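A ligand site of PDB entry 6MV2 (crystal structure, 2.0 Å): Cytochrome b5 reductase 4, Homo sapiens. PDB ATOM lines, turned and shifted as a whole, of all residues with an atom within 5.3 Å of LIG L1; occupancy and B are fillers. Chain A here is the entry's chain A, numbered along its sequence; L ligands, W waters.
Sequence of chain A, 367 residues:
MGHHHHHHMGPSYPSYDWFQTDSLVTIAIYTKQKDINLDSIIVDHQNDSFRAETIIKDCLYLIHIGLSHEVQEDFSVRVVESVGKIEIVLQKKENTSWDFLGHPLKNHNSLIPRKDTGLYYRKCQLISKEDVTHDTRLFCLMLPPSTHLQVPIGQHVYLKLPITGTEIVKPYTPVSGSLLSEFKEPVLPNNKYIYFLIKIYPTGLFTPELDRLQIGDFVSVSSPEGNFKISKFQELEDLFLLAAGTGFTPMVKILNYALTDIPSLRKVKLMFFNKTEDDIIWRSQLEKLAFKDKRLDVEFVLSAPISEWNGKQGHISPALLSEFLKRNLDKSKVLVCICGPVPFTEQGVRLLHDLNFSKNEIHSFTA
OG of Ser 303 sits at hydrogen-bond distance from O17 of LIG L1, at 2.5 Å.
The backbone carbonyl oxygen (O) of Asn 274 is in hydrogen-bond range of an oxygen (O5) of LIG L1 (2.7 Å).
The side-chain hydroxyl (OH) of Tyr 201 sits at hydrogen-bond distance from an oxygen (O8) of LIG L1.
A ring nitrogen (NE2) of His 315 is in hydrogen-bond range of an oxygen (O15) of LIG L1 (2.8 Å).
O9 of LIG L1 lies within salt-bridge range of NZ of Lys 199.
The backbone NH (N) of Thr 246 lies within hydrogen-bond range of an oxygen (O9) of LIG L1 (2.9 Å).
An oxygen (O1) of LIG L1 lies within salt-bridge range of the side-chain amino group (NZ) of Lys 275 (2.9 Å).
SG of Cys 339 lies close to N7 of LIG L1, at 3.8 Å.
The backbone NH (N) of Lys 199 lies within hydrogen-bond range of an oxygen (O7) of LG2 L2.
O8 of LG2 L2 lies within hydrogen-bond range of OG1 of Thr 249, at 2.9 Å.
N of Thr 173 sits at hydrogen-bond distance from O8 of LG2 L2.
N8 of LG2 L2 sits at hydrogen-bond distance from OG1 of Thr 173 (3.2 Å).
N of Ser 303 sits at hydrogen-bond distance from O of Asn 274 (2.8 Å).
The backbone NH of Asn 274 lies within hydrogen-bond range of the backbone carbonyl oxygen of Val 301 (2.9 Å).
The side-chain hydroxyl (OG1) of Thr 249 lies within hydrogen-bond range of the backbone carbonyl oxygen (O) of Thr 246.
N of Ala 304 lies within hydrogen-bond range of O of Lys 275.
N of Ala 244 is in hydrogen-bond range of O of Cys 339 (3.2 Å).
SG of Cys 339 sits at hydrogen-bond distance from O of Phe 365.
The backbone NH (N) of Gly 245 is in hydrogen-bond range of the backbone carbonyl oxygen (O) of Phe 273 (3.0 Å).
O of Gly 340 sits close to O11 of LIG L1, at 3.3 Å.
N of Pro 341 sits close to O11 of LIG L1 (3.5 Å).
An oxygen (O14) of LIG L1 sits close to the backbone carbonyl oxygen of Thr 366, at 3.4 Å.
Thr 173 touches LIG L1 (OG1 to C19, 3.9 Å).
Ala 244 touches LIG L1.
CA of Gly 245 touches O9 of LIG L1, 3.3 Å away.
Gly 247 touches LIG L1.
OG1 of Thr 249 touches C20 of LIG L1, 3.6 Å away.
O of Phe 273 touches C2 of LIG L1, at 3.8 Å.
Pro 343 touches LIG L1.
N of Phe 344 touches N3 of LIG L1 (3.9 Å).
Phe 365 touches LIG L1 (CB to N7, 3.4 Å).
Ala 367 touches LIG L1 (N to O14, 3.7 Å).
Hydrophobic or aromatic side chains within 4 Å of LIG L1: Tyr 201, Ala 244, His 315, Pro 341, Pro 343, Phe 344 and Phe 365.
Water W9 lies within hydrogen-bond range of O1 of LIG L1 (2.5 Å), OD1 of Asn 274 (2.8 Å) and N of Lys 275 (3.0 Å).
Water W6 lies within hydrogen-bond range of the side-chain hydroxyl (OG1) of Thr 173 (2.6 Å) and a nitrogen (N7) of LIG L1 (2.8 Å).
Water W8 bridges N5 of LIG L1 (2.9 Å) and N of Ile 316 (2.9 Å).
Water W10 lies within hydrogen-bond range of O10 of LG2 L2 and O13 of LIG L1.
Water W4 lies within hydrogen-bond range of O14 of LIG L1 (3.2 Å) and O of Gly 340 (3.5 Å).
Water W3 bridges O of Thr 366 (2.7 Å) and N7 of LIG L1 (3.4 Å).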
ATOM      1  N   HIS A 156       8.423  23.055   1.748  1.00  0.00           N
ATOM      2  CA  HIS A 156       8.609  21.646   1.431  1.00  0.00           C
ATOM      3  C   HIS A 156       7.372  20.858   1.859  1.00  0.00           C
ATOM      4  O   HIS A 156       6.491  21.388   2.538  1.00  0.00           O
ATOM      5  CB  HIS A 156       9.853  21.096   2.136  1.00  0.00           C
ATOM      6  CG  HIS A 156       9.933  21.446   3.595  1.00  0.00           C
ATOM      7  ND1 HIS A 156      10.441  22.643   4.045  1.00  0.00           N
ATOM      8  CD2 HIS A 156       9.585  20.744   4.696  1.00  0.00           C
ATOM      9  CE1 HIS A 156      10.385  22.680   5.361  1.00  0.00           C
ATOM     10  NE2 HIS A 156       9.877  21.530   5.784  1.00  0.00           N
ATOM     11  N   THR A 173      11.536  19.440  -1.426  1.00  0.00           N
ATOM     12  CA  THR A 173      11.140  20.796  -1.759  1.00  0.00           C
ATOM     13  C   THR A 173      10.633  20.892  -3.186  1.00  0.00           C
ATOM     14  O   THR A 173      11.451  20.885  -4.119  1.00  0.00           O
ATOM     15  CB  THR A 173      12.321  21.727  -1.573  1.00  0.00           C
ATOM     16  OG1 THR A 173      12.798  21.617  -0.241  1.00  0.00           O
ATOM     17  CG2 THR A 173      11.903  23.191  -1.856  1.00  0.00           C
ATOM     18  N   LYS A 199      17.815  13.439  -5.284  1.00  0.00           N
ATOM     19  CA  LYS A 199      19.057  12.697  -5.437  1.00  0.00           C
ATOM     20  C   LYS A 199      18.882  11.361  -4.728  1.00  0.00           C
ATOM     21  O   LYS A 199      18.390  11.311  -3.598  1.00  0.00           O
ATOM     22  CB  LYS A 199      20.211  13.501  -4.828  1.00  0.00           C
ATOM     23  CG  LYS A 199      21.602  12.804  -4.895  1.00  0.00           C
ATOM     24  CD  LYS A 199      22.789  13.734  -4.496  1.00  0.00           C
ATOM     25  CE  LYS A 199      22.999  14.822  -5.512  1.00  0.00           C
ATOM     26  NZ  LYS A 199      24.148  15.717  -5.192  1.00  0.00           N
ATOM     27  N   TYR A 201      20.505   8.170  -3.007  1.00  0.00           N
ATOM     28  CA  TYR A 201      21.688   7.712  -2.318  1.00  0.00           C
ATOM     29  C   TYR A 201      21.639   6.192  -2.206  1.00  0.00           C
ATOM     30  O   TYR A 201      20.769   5.664  -1.503  1.00  0.00           O
ATOM     31  CB  TYR A 201      21.772   8.326  -0.933  1.00  0.00           C
ATOM     32  CG  TYR A 201      21.824   9.845  -0.933  1.00  0.00           C
ATOM     33  CD1 TYR A 201      23.033  10.539  -1.043  1.00  0.00           C
ATOM     34  CD2 TYR A 201      20.652  10.581  -0.839  1.00  0.00           C
ATOM     35  CE1 TYR A 201      23.072  11.941  -1.034  1.00  0.00           C
ATOM     36  CE2 TYR A 201      20.678  11.978  -0.831  1.00  0.00           C
ATOM     37  CZ  TYR A 201      21.889  12.646  -0.926  1.00  0.00           C
ATOM     38  OH  TYR A 201      21.893  14.041  -0.919  1.00  0.00           O
ATOM     39  N   ALA A 244      24.351  24.341  -2.630  1.00  0.00           N
ATOM     40  CA  ALA A 244      25.219  23.184  -2.751  1.00  0.00           C
ATOM     41  C   ALA A 244      24.360  21.951  -2.987  1.00  0.00           C
ATOM     42  O   ALA A 244      23.526  21.593  -2.161  1.00  0.00           O
ATOM     43  CB  ALA A 244      26.068  22.986  -1.490  1.00  0.00           C
ATOM     44  N   GLY A 245      24.604  21.277  -4.105  1.00  0.00           N
ATOM     45  CA  GLY A 245      23.991  19.987  -4.321  1.00  0.00           C
ATOM     46  C   GLY A 245      22.497  20.156  -4.474  1.00  0.00           C
ATOM     47  O   GLY A 245      22.032  21.083  -5.151  1.00  0.00           O
ATOM     48  N   THR A 246      21.736  19.280  -3.829  1.00  0.00           N
ATOM     49  CA  THR A 246      20.285  19.415  -3.896  1.00  0.00           C
ATOM     50  C   THR A 246      19.777  20.624  -3.140  1.00  0.00           C
ATOM     51  O   THR A 246      18.562  20.840  -3.142  1.00  0.00           O
ATOM     52  CB  THR A 246      19.581  18.165  -3.346  1.00  0.00           C
ATOM     53  OG1 THR A 246      19.819  18.069  -1.940  1.00  0.00           O
ATOM     54  CG2 THR A 246      20.067  16.894  -4.022  1.00  0.00           C
ATOM     55  N   GLY A 247      20.647  21.411  -2.485  1.00  0.00           N
ATOM     56  CA  GLY A 247      20.225  22.725  -1.993  1.00  0.00           C
ATOM     57  C   GLY A 247      19.797  23.665  -3.092  1.00  0.00           C
ATOM     58  O   GLY A 247      19.298  24.767  -2.813  1.00  0.00           O
ATOM     59  N   THR A 249      17.232  22.933  -4.865  1.00  0.00           N
ATOM     60  CA  THR A 249      15.792  22.806  -5.120  1.00  0.00           C
ATOM     61  C   THR A 249      14.941  24.009  -4.655  1.00  0.00           C
ATOM     62  O   THR A 249      14.083  24.455  -5.434  1.00  0.00           O
ATOM     63  CB  THR A 249      15.252  21.483  -4.587  1.00  0.00           C
ATOM     64  OG1 THR A 249      15.369  21.377  -3.167  1.00  0.00           O
ATOM     65  CG2 THR A 249      16.011  20.334  -5.260  1.00  0.00           C
ATOM     66  N   PRO A 250      15.075  24.571  -3.440  1.00  0.00           N
ATOM     67  CA  PRO A 250      14.271  25.800  -3.141  1.00  0.00           C
ATOM     68  C   PRO A 250      14.570  26.944  -4.062  1.00  0.00           C
ATOM     69  O   PRO A 250      13.720  27.837  -4.242  1.00  0.00           O
ATOM     70  CB  PRO A 250      14.652  26.152  -1.689  1.00  0.00           C
ATOM     71  CG  PRO A 250      15.931  25.390  -1.417  1.00  0.00           C
ATOM     72  CD  PRO A 250      15.854  24.142  -2.254  1.00  0.00           C
ATOM     73  N   PHE A 273      27.395  25.155  -5.917  1.00  0.00           N
ATOM     74  CA  PHE A 273      28.526  24.308  -5.534  1.00  0.00           C
ATOM     75  C   PHE A 273      28.179  22.843  -5.720  1.00  0.00           C
ATOM     76  O   PHE A 273      27.109  22.402  -5.284  1.00  0.00           O
ATOM     77  CB  PHE A 273      28.924  24.509  -4.068  1.00  0.00           C
ATOM     78  CG  PHE A 273      29.316  25.912  -3.708  1.00  0.00           C
ATOM     79  CD1 PHE A 273      28.347  26.884  -3.493  1.00  0.00           C
ATOM     80  CD2 PHE A 273      30.640  26.243  -3.533  1.00  0.00           C
ATOM     81  CE1 PHE A 273      28.721  28.183  -3.122  1.00  0.00           C
ATOM     82  CE2 PHE A 273      31.016  27.520  -3.167  1.00  0.00           C
ATOM     83  CZ  PHE A 273      30.056  28.488  -2.951  1.00  0.00           C
ATOM     84  N   ASN A 274      29.090  22.080  -6.327  1.00  0.00           N
ATOM     85  CA  ASN A 274      28.903  20.643  -6.532  1.00  0.00           C
ATOM     86  C   ASN A 274      30.272  19.962  -6.465  1.00  0.00           C
ATOM     87  O   ASN A 274      31.317  20.601  -6.307  1.00  0.00           O
ATOM     88  CB  ASN A 274      28.214  20.344  -7.865  1.00  0.00           C
ATOM     89  CG  ASN A 274      26.713  20.621  -7.826  1.00  0.00           C
ATOM     90  OD1 ASN A 274      25.960  19.902  -7.163  1.00  0.00           O
ATOM     91  ND2 ASN A 274      26.270  21.636  -8.557  1.00  0.00           N
ATOM     92  N   LYS A 275      30.249  18.635  -6.562  1.00  0.00           N
ATOM     93  CA  LYS A 275      31.477  17.845  -6.551  1.00  0.00           C
ATOM     94  C   LYS A 275      32.130  17.803  -7.925  1.00  0.00           C
ATOM     95  O   LYS A 275      33.284  18.248  -8.102  1.00  0.00           O
ATOM     96  CB  LYS A 275      31.149  16.434  -6.045  1.00  0.00           C
ATOM     97  CG  LYS A 275      30.583  16.420  -4.617  1.00  0.00           C
ATOM     98  CD  LYS A 275      30.549  15.037  -3.952  1.00  0.00           C
ATOM     99  CE  LYS A 275      29.670  14.038  -4.676  1.00  0.00           C
ATOM    100  NZ  LYS A 275      28.204  14.223  -4.408  1.00  0.00           N
ATOM    101  N   VAL A 301      30.845  26.203  -9.043  1.00  0.00           N
ATOM    102  CA  VAL A 301      32.033  25.891  -8.267  1.00  0.00           C
ATOM    103  C   VAL A 301      32.064  24.375  -8.060  1.00  0.00           C
ATOM    104  O   VAL A 301      31.077  23.789  -7.606  1.00  0.00           O
ATOM    105  CB  VAL A 301      32.037  26.606  -6.908  1.00  0.00           C
ATOM    106  CG1 VAL A 301      33.318  26.256  -6.125  1.00  0.00           C
ATOM    107  CG2 VAL A 301      31.879  28.123  -7.090  1.00  0.00           C
ATOM    108  N   SER A 303      34.076  21.181  -6.211  1.00  0.00           N
ATOM    109  CA  SER A 303      34.998  20.798  -5.154  1.00  0.00           C
ATOM    110  C   SER A 303      35.984  19.719  -5.581  1.00  0.00           C
ATOM    111  O   SER A 303      37.075  19.615  -5.006  1.00  0.00           O
ATOM    112  CB  SER A 303      34.208  20.305  -3.953  1.00  0.00           C
ATOM    113  OG  SER A 303      33.314  19.272  -4.358  1.00  0.00           O
ATOM    114  N   ALA A 304      35.629  18.928  -6.572  1.00  0.00           N
ATOM    115  CA  ALA A 304      36.432  17.757  -6.891  1.00  0.00           C
ATOM    116  C   ALA A 304      36.312  17.415  -8.360  1.00  0.00           C
ATOM    117  O   ALA A 304      35.949  16.281  -8.701  1.00  0.00           O
ATOM    118  CB  ALA A 304      35.988  16.576  -6.043  1.00  0.00           C
ATOM    119  N   GLY A 314      36.615  24.571  -5.305  1.00  0.00           N
ATOM    120  CA  GLY A 314      36.704  24.669  -3.860  1.00  0.00           C
ATOM    121  C   GLY A 314      35.382  24.554  -3.132  1.00  0.00           C
ATOM    122  O   GLY A 314      34.423  23.969  -3.632  1.00  0.00           O
ATOM    123  N   HIS A 315      35.362  25.078  -1.920  1.00  0.00           N
ATOM    124  CA  HIS A 315      34.187  25.113  -1.078  1.00  0.00           C
ATOM    125  C   HIS A 315      33.888  26.559  -0.729  1.00  0.00           C
ATOM    126  O   HIS A 315      34.723  27.457  -0.910  1.00  0.00           O
ATOM    127  CB  HIS A 315      34.388  24.293   0.197  1.00  0.00           C
ATOM    128  CG  HIS A 315      34.786  22.874  -0.052  1.00  0.00           C
ATOM    129  ND1 HIS A 315      35.972  22.517  -0.657  1.00  0.00           N
ATOM    130  CD2 HIS A 315      34.149  21.705   0.231  1.00  0.00           C
ATOM    131  CE1 HIS A 315      36.038  21.200  -0.758  1.00  0.00           C
ATOM    132  NE2 HIS A 315      34.952  20.681  -0.225  1.00  0.00           N
ATOM    133  N   ILE A 316      32.688  26.774  -0.201  1.00  0.00           N
ATOM    134  CA  ILE A 316      32.303  28.103   0.255  1.00  0.00           C
ATOM    135  C   ILE A 316      33.371  28.631   1.218  1.00  0.00           C
ATOM    136  O   ILE A 316      33.760  27.934   2.156  1.00  0.00           O
ATOM    137  CB  ILE A 316      30.917  28.049   0.910  1.00  0.00           C
ATOM    138  CG1 ILE A 316      30.364  29.459   1.120  1.00  0.00           C
ATOM    139  CG2 ILE A 316      30.951  27.267   2.215  1.00  0.00           C
ATOM    140  CD1 ILE A 316      28.858  29.522   1.252  1.00  0.00           C
ATOM    141  N   CYS A 339      21.213  27.399   0.819  1.00  0.00           N
ATOM    142  CA  CYS A 339      20.720  26.075   1.151  1.00  0.00           C
ATOM    143  C   CYS A 339      21.772  25.054   0.747  1.00  0.00           C
ATOM    144  O   CYS A 339      22.453  25.224  -0.262  1.00  0.00           O
ATOM    145  CB  CYS A 339      19.385  25.752   0.458  1.00  0.00           C
ATOM    146  SG  CYS A 339      18.608  24.180   0.957  1.00  0.00           S
ATOM    147  N   GLY A 340      21.894  24.009   1.541  1.00  0.00           N
ATOM    148  CA  GLY A 340      22.846  22.968   1.271  1.00  0.00           C
ATOM    149  C   GLY A 340      22.968  22.034   2.451  1.00  0.00           C
ATOM    150  O   GLY A 340      22.109  22.024   3.329  1.00  0.00           O
ATOM    151  N   PRO A 341      24.026  21.218   2.490  1.00  0.00           N
ATOM    152  CA  PRO A 341      24.338  20.493   3.726  1.00  0.00           C
ATOM    153  C   PRO A 341      24.407  21.443   4.926  1.00  0.00           C
ATOM    154  O   PRO A 341      24.790  22.607   4.795  1.00  0.00           O
ATOM    155  CB  PRO A 341      25.701  19.851   3.433  1.00  0.00           C
ATOM    156  CG  PRO A 341      25.749  19.725   1.918  1.00  0.00           C
ATOM    157  CD  PRO A 341      24.987  20.951   1.425  1.00  0.00           C
ATOM    158  N   VAL A 342      23.967  20.943   6.079  1.00  0.00           N
ATOM    159  CA  VAL A 342      23.844  21.784   7.272  1.00  0.00           C
ATOM    160  C   VAL A 342      25.126  22.555   7.565  1.00  0.00           C
ATOM    161  O   VAL A 342      25.058  23.778   7.761  1.00  0.00           O
ATOM    162  CB  VAL A 342      23.387  20.933   8.463  1.00  0.00           C
ATOM    163  CG1 VAL A 342      23.663  21.633   9.800  1.00  0.00           C
ATOM    164  CG2 VAL A 342      21.871  20.602   8.341  1.00  0.00           C
ATOM    165  N   PRO A 343      26.305  21.937   7.635  1.00  0.00           N
ATOM    166  CA  PRO A 343      27.510  22.732   7.909  1.00  0.00           C
ATOM    167  C   PRO A 343      27.811  23.754   6.824  1.00  0.00           C
ATOM    168  O   PRO A 343      28.281  24.863   7.134  1.00  0.00           O
ATOM    169  CB  PRO A 343      28.607  21.649   8.004  1.00  0.00           C
ATOM    170  CG  PRO A 343      28.035  20.441   7.347  1.00  0.00           C
ATOM    171  CD  PRO A 343      26.571  20.492   7.621  1.00  0.00           C
ATOM    172  N   PHE A 344      27.558  23.412   5.562  1.00  0.00           N
ATOM    173  CA  PHE A 344      27.707  24.374   4.480  1.00  0.00           C
ATOM    174  C   PHE A 344      26.848  25.602   4.726  1.00  0.00           C
ATOM    175  O   PHE A 344      27.277  26.731   4.458  1.00  0.00           O
ATOM    176  CB  PHE A 344      27.354  23.726   3.139  1.00  0.00           C
ATOM    177  CG  PHE A 344      27.096  24.693   2.011  1.00  0.00           C
ATOM    178  CD1 PHE A 344      25.840  25.286   1.831  1.00  0.00           C
ATOM    179  CD2 PHE A 344      28.083  24.955   1.092  1.00  0.00           C
ATOM    180  CE1 PHE A 344      25.609  26.151   0.777  1.00  0.00           C
ATOM    181  CE2 PHE A 344      27.856  25.830   0.030  1.00  0.00           C
ATOM    182  CZ  PHE A 344      26.614  26.404  -0.132  1.00  0.00           C
ATOM    183  N   PHE A 365      17.654  28.077   4.159  1.00  0.00           N
ATOM    184  CA  PHE A 365      16.691  26.981   4.106  1.00  0.00           C
ATOM    185  C   PHE A 365      17.257  25.785   4.840  1.00  0.00           C
ATOM    186  O   PHE A 365      18.303  25.245   4.441  1.00  0.00           O
ATOM    187  CB  PHE A 365      16.367  26.636   2.668  1.00  0.00           C
ATOM    188  CG  PHE A 365      15.585  27.659   1.965  1.00  0.00           C
ATOM    189  CD1 PHE A 365      14.211  27.675   2.074  1.00  0.00           C
ATOM    190  CD2 PHE A 365      16.198  28.579   1.169  1.00  0.00           C
ATOM    191  CE1 PHE A 365      13.455  28.626   1.410  1.00  0.00           C
ATOM    192  CE2 PHE A 365      15.455  29.535   0.507  1.00  0.00           C
ATOM    193  CZ  PHE A 365      14.067  29.542   0.634  1.00  0.00           C
ATOM    194  N   THR A 366      16.577  25.365   5.896  1.00  0.00           N
ATOM    195  CA  THR A 366      16.985  24.251   6.750  1.00  0.00           C
ATOM    196  C   THR A 366      15.728  23.468   7.137  1.00  0.00           C
ATOM    197  O   THR A 366      14.626  23.733   6.651  1.00  0.00           O
ATOM    198  CB  THR A 366      17.756  24.768   7.973  1.00  0.00           C
ATOM    199  OG1 THR A 366      16.970  25.764   8.647  1.00  0.00           O
ATOM    200  CG2 THR A 366      19.087  25.354   7.553  1.00  0.00           C
ATOM    201  N   ALA A 367      15.886  22.509   8.039  1.00  0.00           N
ATOM    202  CA  ALA A 367      14.749  21.675   8.442  1.00  0.00           C
ATOM    203  C   ALA A 367      13.716  22.498   9.208  1.00  0.00           C
ATOM    204  O   ALA A 367      12.562  22.596   8.791  1.00  0.00           O
ATOM    205  CB  ALA A 367      15.217  20.494   9.297  1.00  0.00           C
HETATM  206  P1  LIG L   1      26.845  16.901  -2.255  1.00  0.00           P
HETATM  207  O1  LIG L   1      26.798  16.721  -3.754  1.00  0.00           O
HETATM  208  O2  LIG L   1      27.386  15.722  -1.499  1.00  0.00           O
HETATM  209  O3  LIG L   1      27.813  18.162  -1.989  1.00  0.00           O
HETATM  210  C1  LIG L   1      27.470  19.398  -2.595  1.00  0.00           C
HETATM  211  C2  LIG L   1      28.647  20.354  -2.476  1.00  0.00           C
HETATM  212  O4  LIG L   1      28.696  20.883  -1.149  1.00  0.00           O
HETATM  213  C3  LIG L   1      29.991  19.659  -2.739  1.00  0.00           C
HETATM  214  O5  LIG L   1      30.745  20.508  -3.623  1.00  0.00           O
HETATM  215  C4  LIG L   1      30.572  19.452  -1.338  1.00  0.00           C
HETATM  216  O6  LIG L   1      32.005  19.374  -1.191  1.00  0.00           O
HETATM  217  C5  LIG L   1      30.008  20.657  -0.617  1.00  0.00           C
HETATM  218  N1  LIG L   1      29.986  20.412   0.843  1.00  0.00           N
HETATM  219  C6  LIG L   1      29.485  19.346   1.496  1.00  0.00           C
HETATM  220  N2  LIG L   1      29.652  19.487   2.840  1.00  0.00           N
HETATM  221  C7  LIG L   1      30.272  20.658   3.035  1.00  0.00           C
HETATM  222  C8  LIG L   1      30.759  21.418   4.198  1.00  0.00           C
HETATM  223  N3  LIG L   1      30.608  20.936   5.457  1.00  0.00           N
HETATM  224  N4  LIG L   1      31.366  22.613   3.960  1.00  0.00           N
HETATM  225  C9  LIG L   1      31.523  23.110   2.723  1.00  0.00           C
HETATM  226  N5  LIG L   1      31.103  22.466   1.614  1.00  0.00           N
HETATM  227  C10 LIG L   1      30.488  21.257   1.717  1.00  0.00           C
HETATM  228  O7  LIG L   1      25.474  17.470  -1.630  1.00  0.00           O
HETATM  229  P2  LIG L   1      24.064  16.706  -1.592  1.00  0.00           P
HETATM  230  O8  LIG L   1      24.331  15.222  -1.410  1.00  0.00           O
HETATM  231  O9  LIG L   1      23.323  17.100  -2.843  1.00  0.00           O
HETATM  232  O10 LIG L   1      23.276  17.209  -0.294  1.00  0.00           O
HETATM  233  C11 LIG L   1      22.737  18.530  -0.272  1.00  0.00           C
HETATM  234  C12 LIG L   1      22.132  18.781   1.110  1.00  0.00           C
HETATM  235  O11 LIG L   1      21.190  19.844   1.028  1.00  0.00           O
HETATM  236  C13 LIG L   1      21.373  17.605   1.722  1.00  0.00           C
HETATM  237  O12 LIG L   1      21.961  17.397   3.000  1.00  0.00           O
HETATM  238  C14 LIG L   1      19.943  18.057   1.887  1.00  0.00           C
HETATM  239  O13 LIG L   1      19.330  17.606   3.082  1.00  0.00           O
HETATM  240  C15 LIG L   1      20.092  19.576   1.921  1.00  0.00           C
HETATM  241  N6  LIG L   1      18.867  20.235   1.511  1.00  0.00           N
HETATM  242  C16 LIG L   1      18.200  20.939   2.433  1.00  0.00           C
HETATM  243  C17 LIG L   1      17.017  21.593   2.136  1.00  0.00           C
HETATM  244  C18 LIG L   1      16.357  22.354   3.252  1.00  0.00           C
HETATM  245  O14 LIG L   1      16.614  22.102   4.417  1.00  0.00           O
HETATM  246  N7  LIG L   1      15.534  23.327   2.945  1.00  0.00           N
HETATM  247  C19 LIG L   1      16.498  21.534   0.853  1.00  0.00           C
HETATM  248  C20 LIG L   1      17.149  20.794  -0.128  1.00  0.00           C
HETATM  249  C21 LIG L   1      18.396  20.089   0.133  1.00  0.00           C
HETATM  250  P3  LIG L   1      32.775  17.947  -1.080  1.00  0.00           P
HETATM  251  O15 LIG L   1      33.960  18.086  -0.152  1.00  0.00           O
HETATM  252  O16 LIG L   1      31.895  16.828  -0.575  1.00  0.00           O
HETATM  253  O17 LIG L   1      33.234  17.626  -2.481  1.00  0.00           O
HETATM  254  P1  LG2 L   2      19.743   8.734   4.455  1.00  0.00           P
HETATM  255  O1  LG2 L   2      19.391   7.370   4.989  1.00  0.00           O
HETATM  256  O2  LG2 L   2      19.255   9.818   5.362  1.00  0.00           O
HETATM  257  O3  LG2 L   2      21.321   8.861   4.269  1.00  0.00           O
HETATM  258  C1  LG2 L   2      21.896   8.890   2.966  1.00  0.00           C
HETATM  259  C2  LG2 L   2      23.400   8.671   3.019  1.00  0.00           C
HETATM  260  O4  LG2 L   2      24.052   9.931   3.140  1.00  0.00           O
HETATM  261  C3  LG2 L   2      23.895   7.841   4.203  1.00  0.00           C
HETATM  262  O5  LG2 L   2      23.947   6.443   3.933  1.00  0.00           O
HETATM  263  C4  LG2 L   2      25.277   8.402   4.421  1.00  0.00           C
HETATM  264  O6  LG2 L   2      26.201   7.809   3.479  1.00  0.00           O
HETATM  265  C5  LG2 L   2      25.050   9.884   4.170  1.00  0.00           C
HETATM  266  N1  LG2 L   2      24.595  10.557   5.441  1.00  0.00           N
HETATM  267  C6  LG2 L   2      23.356  10.530   5.995  1.00  0.00           C
HETATM  268  N2  LG2 L   2      23.300  11.246   7.138  1.00  0.00           N
HETATM  269  C7  LG2 L   2      24.525  11.762   7.342  1.00  0.00           C
HETATM  270  C8  LG2 L   2      25.143  12.617   8.375  1.00  0.00           C
HETATM  271  N3  LG2 L   2      24.426  13.073   9.434  1.00  0.00           N
HETATM  272  N4  LG2 L   2      26.452  12.907   8.227  1.00  0.00           N
HETATM  273  C9  LG2 L   2      27.175  12.468   7.182  1.00  0.00           C
HETATM  274  N5  LG2 L   2      26.664  11.691   6.208  1.00  0.00           N
HETATM  275  C10 LG2 L   2      25.366  11.301   6.227  1.00  0.00           C
HETATM  276  N6  LG2 L   2      16.674  16.076  -0.902  1.00  0.00           N
HETATM  277  C11 LG2 L   2      16.490  16.114  -2.235  1.00  0.00           C
HETATM  278  O7  LG2 L   2      17.059  15.279  -2.961  1.00  0.00           O
HETATM  279  N7  LG2 L   2      15.683  17.034  -2.805  1.00  0.00           N
HETATM  280  C12 LG2 L   2      15.014  17.973  -2.135  1.00  0.00           C
HETATM  281  O8  LG2 L   2      14.270  18.782  -2.712  1.00  0.00           O
HETATM  282  C13 LG2 L   2      15.156  18.014  -0.678  1.00  0.00           C
HETATM  283  N8  LG2 L   2      14.516  18.936   0.081  1.00  0.00           N
HETATM  284  C14 LG2 L   2      14.711  18.900   1.435  1.00  0.00           C
HETATM  285  C15 LG2 L   2      14.071  19.848   2.229  1.00  0.00           C
HETATM  286  C16 LG2 L   2      14.230  19.854   3.610  1.00  0.00           C
HETATM  287  C17 LG2 L   2      13.497  20.893   4.457  1.00  0.00           C
HETATM  288  C18 LG2 L   2      15.139  18.858   4.252  1.00  0.00           C
HETATM  289  C19 LG2 L   2      15.344  18.836   5.741  1.00  0.00           C
HETATM  290  C20 LG2 L   2      15.794  17.892   3.465  1.00  0.00           C
HETATM  291  C21 LG2 L   2      15.622  17.881   2.083  1.00  0.00           C
HETATM  292  N9  LG2 L   2      16.273  16.933   1.269  1.00  0.00           N
HETATM  293  C22 LG2 L   2      16.063  16.989  -0.103  1.00  0.00           C
HETATM  294  C23 LG2 L   2      17.121  15.843   1.789  1.00  0.00           C
HETATM  295  C24 LG2 L   2      16.107  14.706   1.991  1.00  0.00           C
HETATM  296  O9  LG2 L   2      15.125  15.065   2.960  1.00  0.00           O
HETATM  297  C25 LG2 L   2      16.685  13.390   2.531  1.00  0.00           C
HETATM  298  O10 LG2 L   2      17.512  13.642   3.658  1.00  0.00           O
HETATM  299  C26 LG2 L   2      17.500  12.688   1.473  1.00  0.00           C
HETATM  300  O11 LG2 L   2      16.576  12.345   0.448  1.00  0.00           O
HETATM  301  C27 LG2 L   2      18.227  11.452   2.033  1.00  0.00           C
HETATM  302  O12 LG2 L   2      17.303  10.545   2.605  1.00  0.00           O
HETATM  303  P2  LG2 L   2      17.601   8.964   2.557  1.00  0.00           P
HETATM  304  O13 LG2 L   2      16.776   8.228   3.561  1.00  0.00           O
HETATM  305  O14 LG2 L   2      17.486   8.463   1.161  1.00  0.00           O
HETATM  306  O15 LG2 L   2      19.174   8.871   2.941  1.00  0.00           O
HETATM  307  O   HOH W   1      28.043  17.969   5.063  1.00  0.00           O
HETATM  308  O   HOH W   2      29.503  16.454   0.001  1.00  0.00           O
HETATM  309  O   HOH W   3      13.666  25.433   4.801  1.00  0.00           O
HETATM  310  O   HOH W   4      19.520  21.161   5.517  1.00  0.00           O
HETATM  311  O   HOH W   5      31.774  23.072  -3.110  1.00  0.00           O
HETATM  312  O   HOH W   6      13.580  23.795   1.016  1.00  0.00           O
HETATM  313  O   HOH W   7      19.907  18.402   5.780  1.00  0.00           O
HETATM  314  O   HOH W   8      31.194  24.278  -0.630  1.00  0.00           O
HETATM  315  O   HOH W   9      27.426  17.784  -5.977  1.00  0.00           O
HETATM  316  O   HOH W  10      20.227  14.759   3.218  1.00  0.00           O
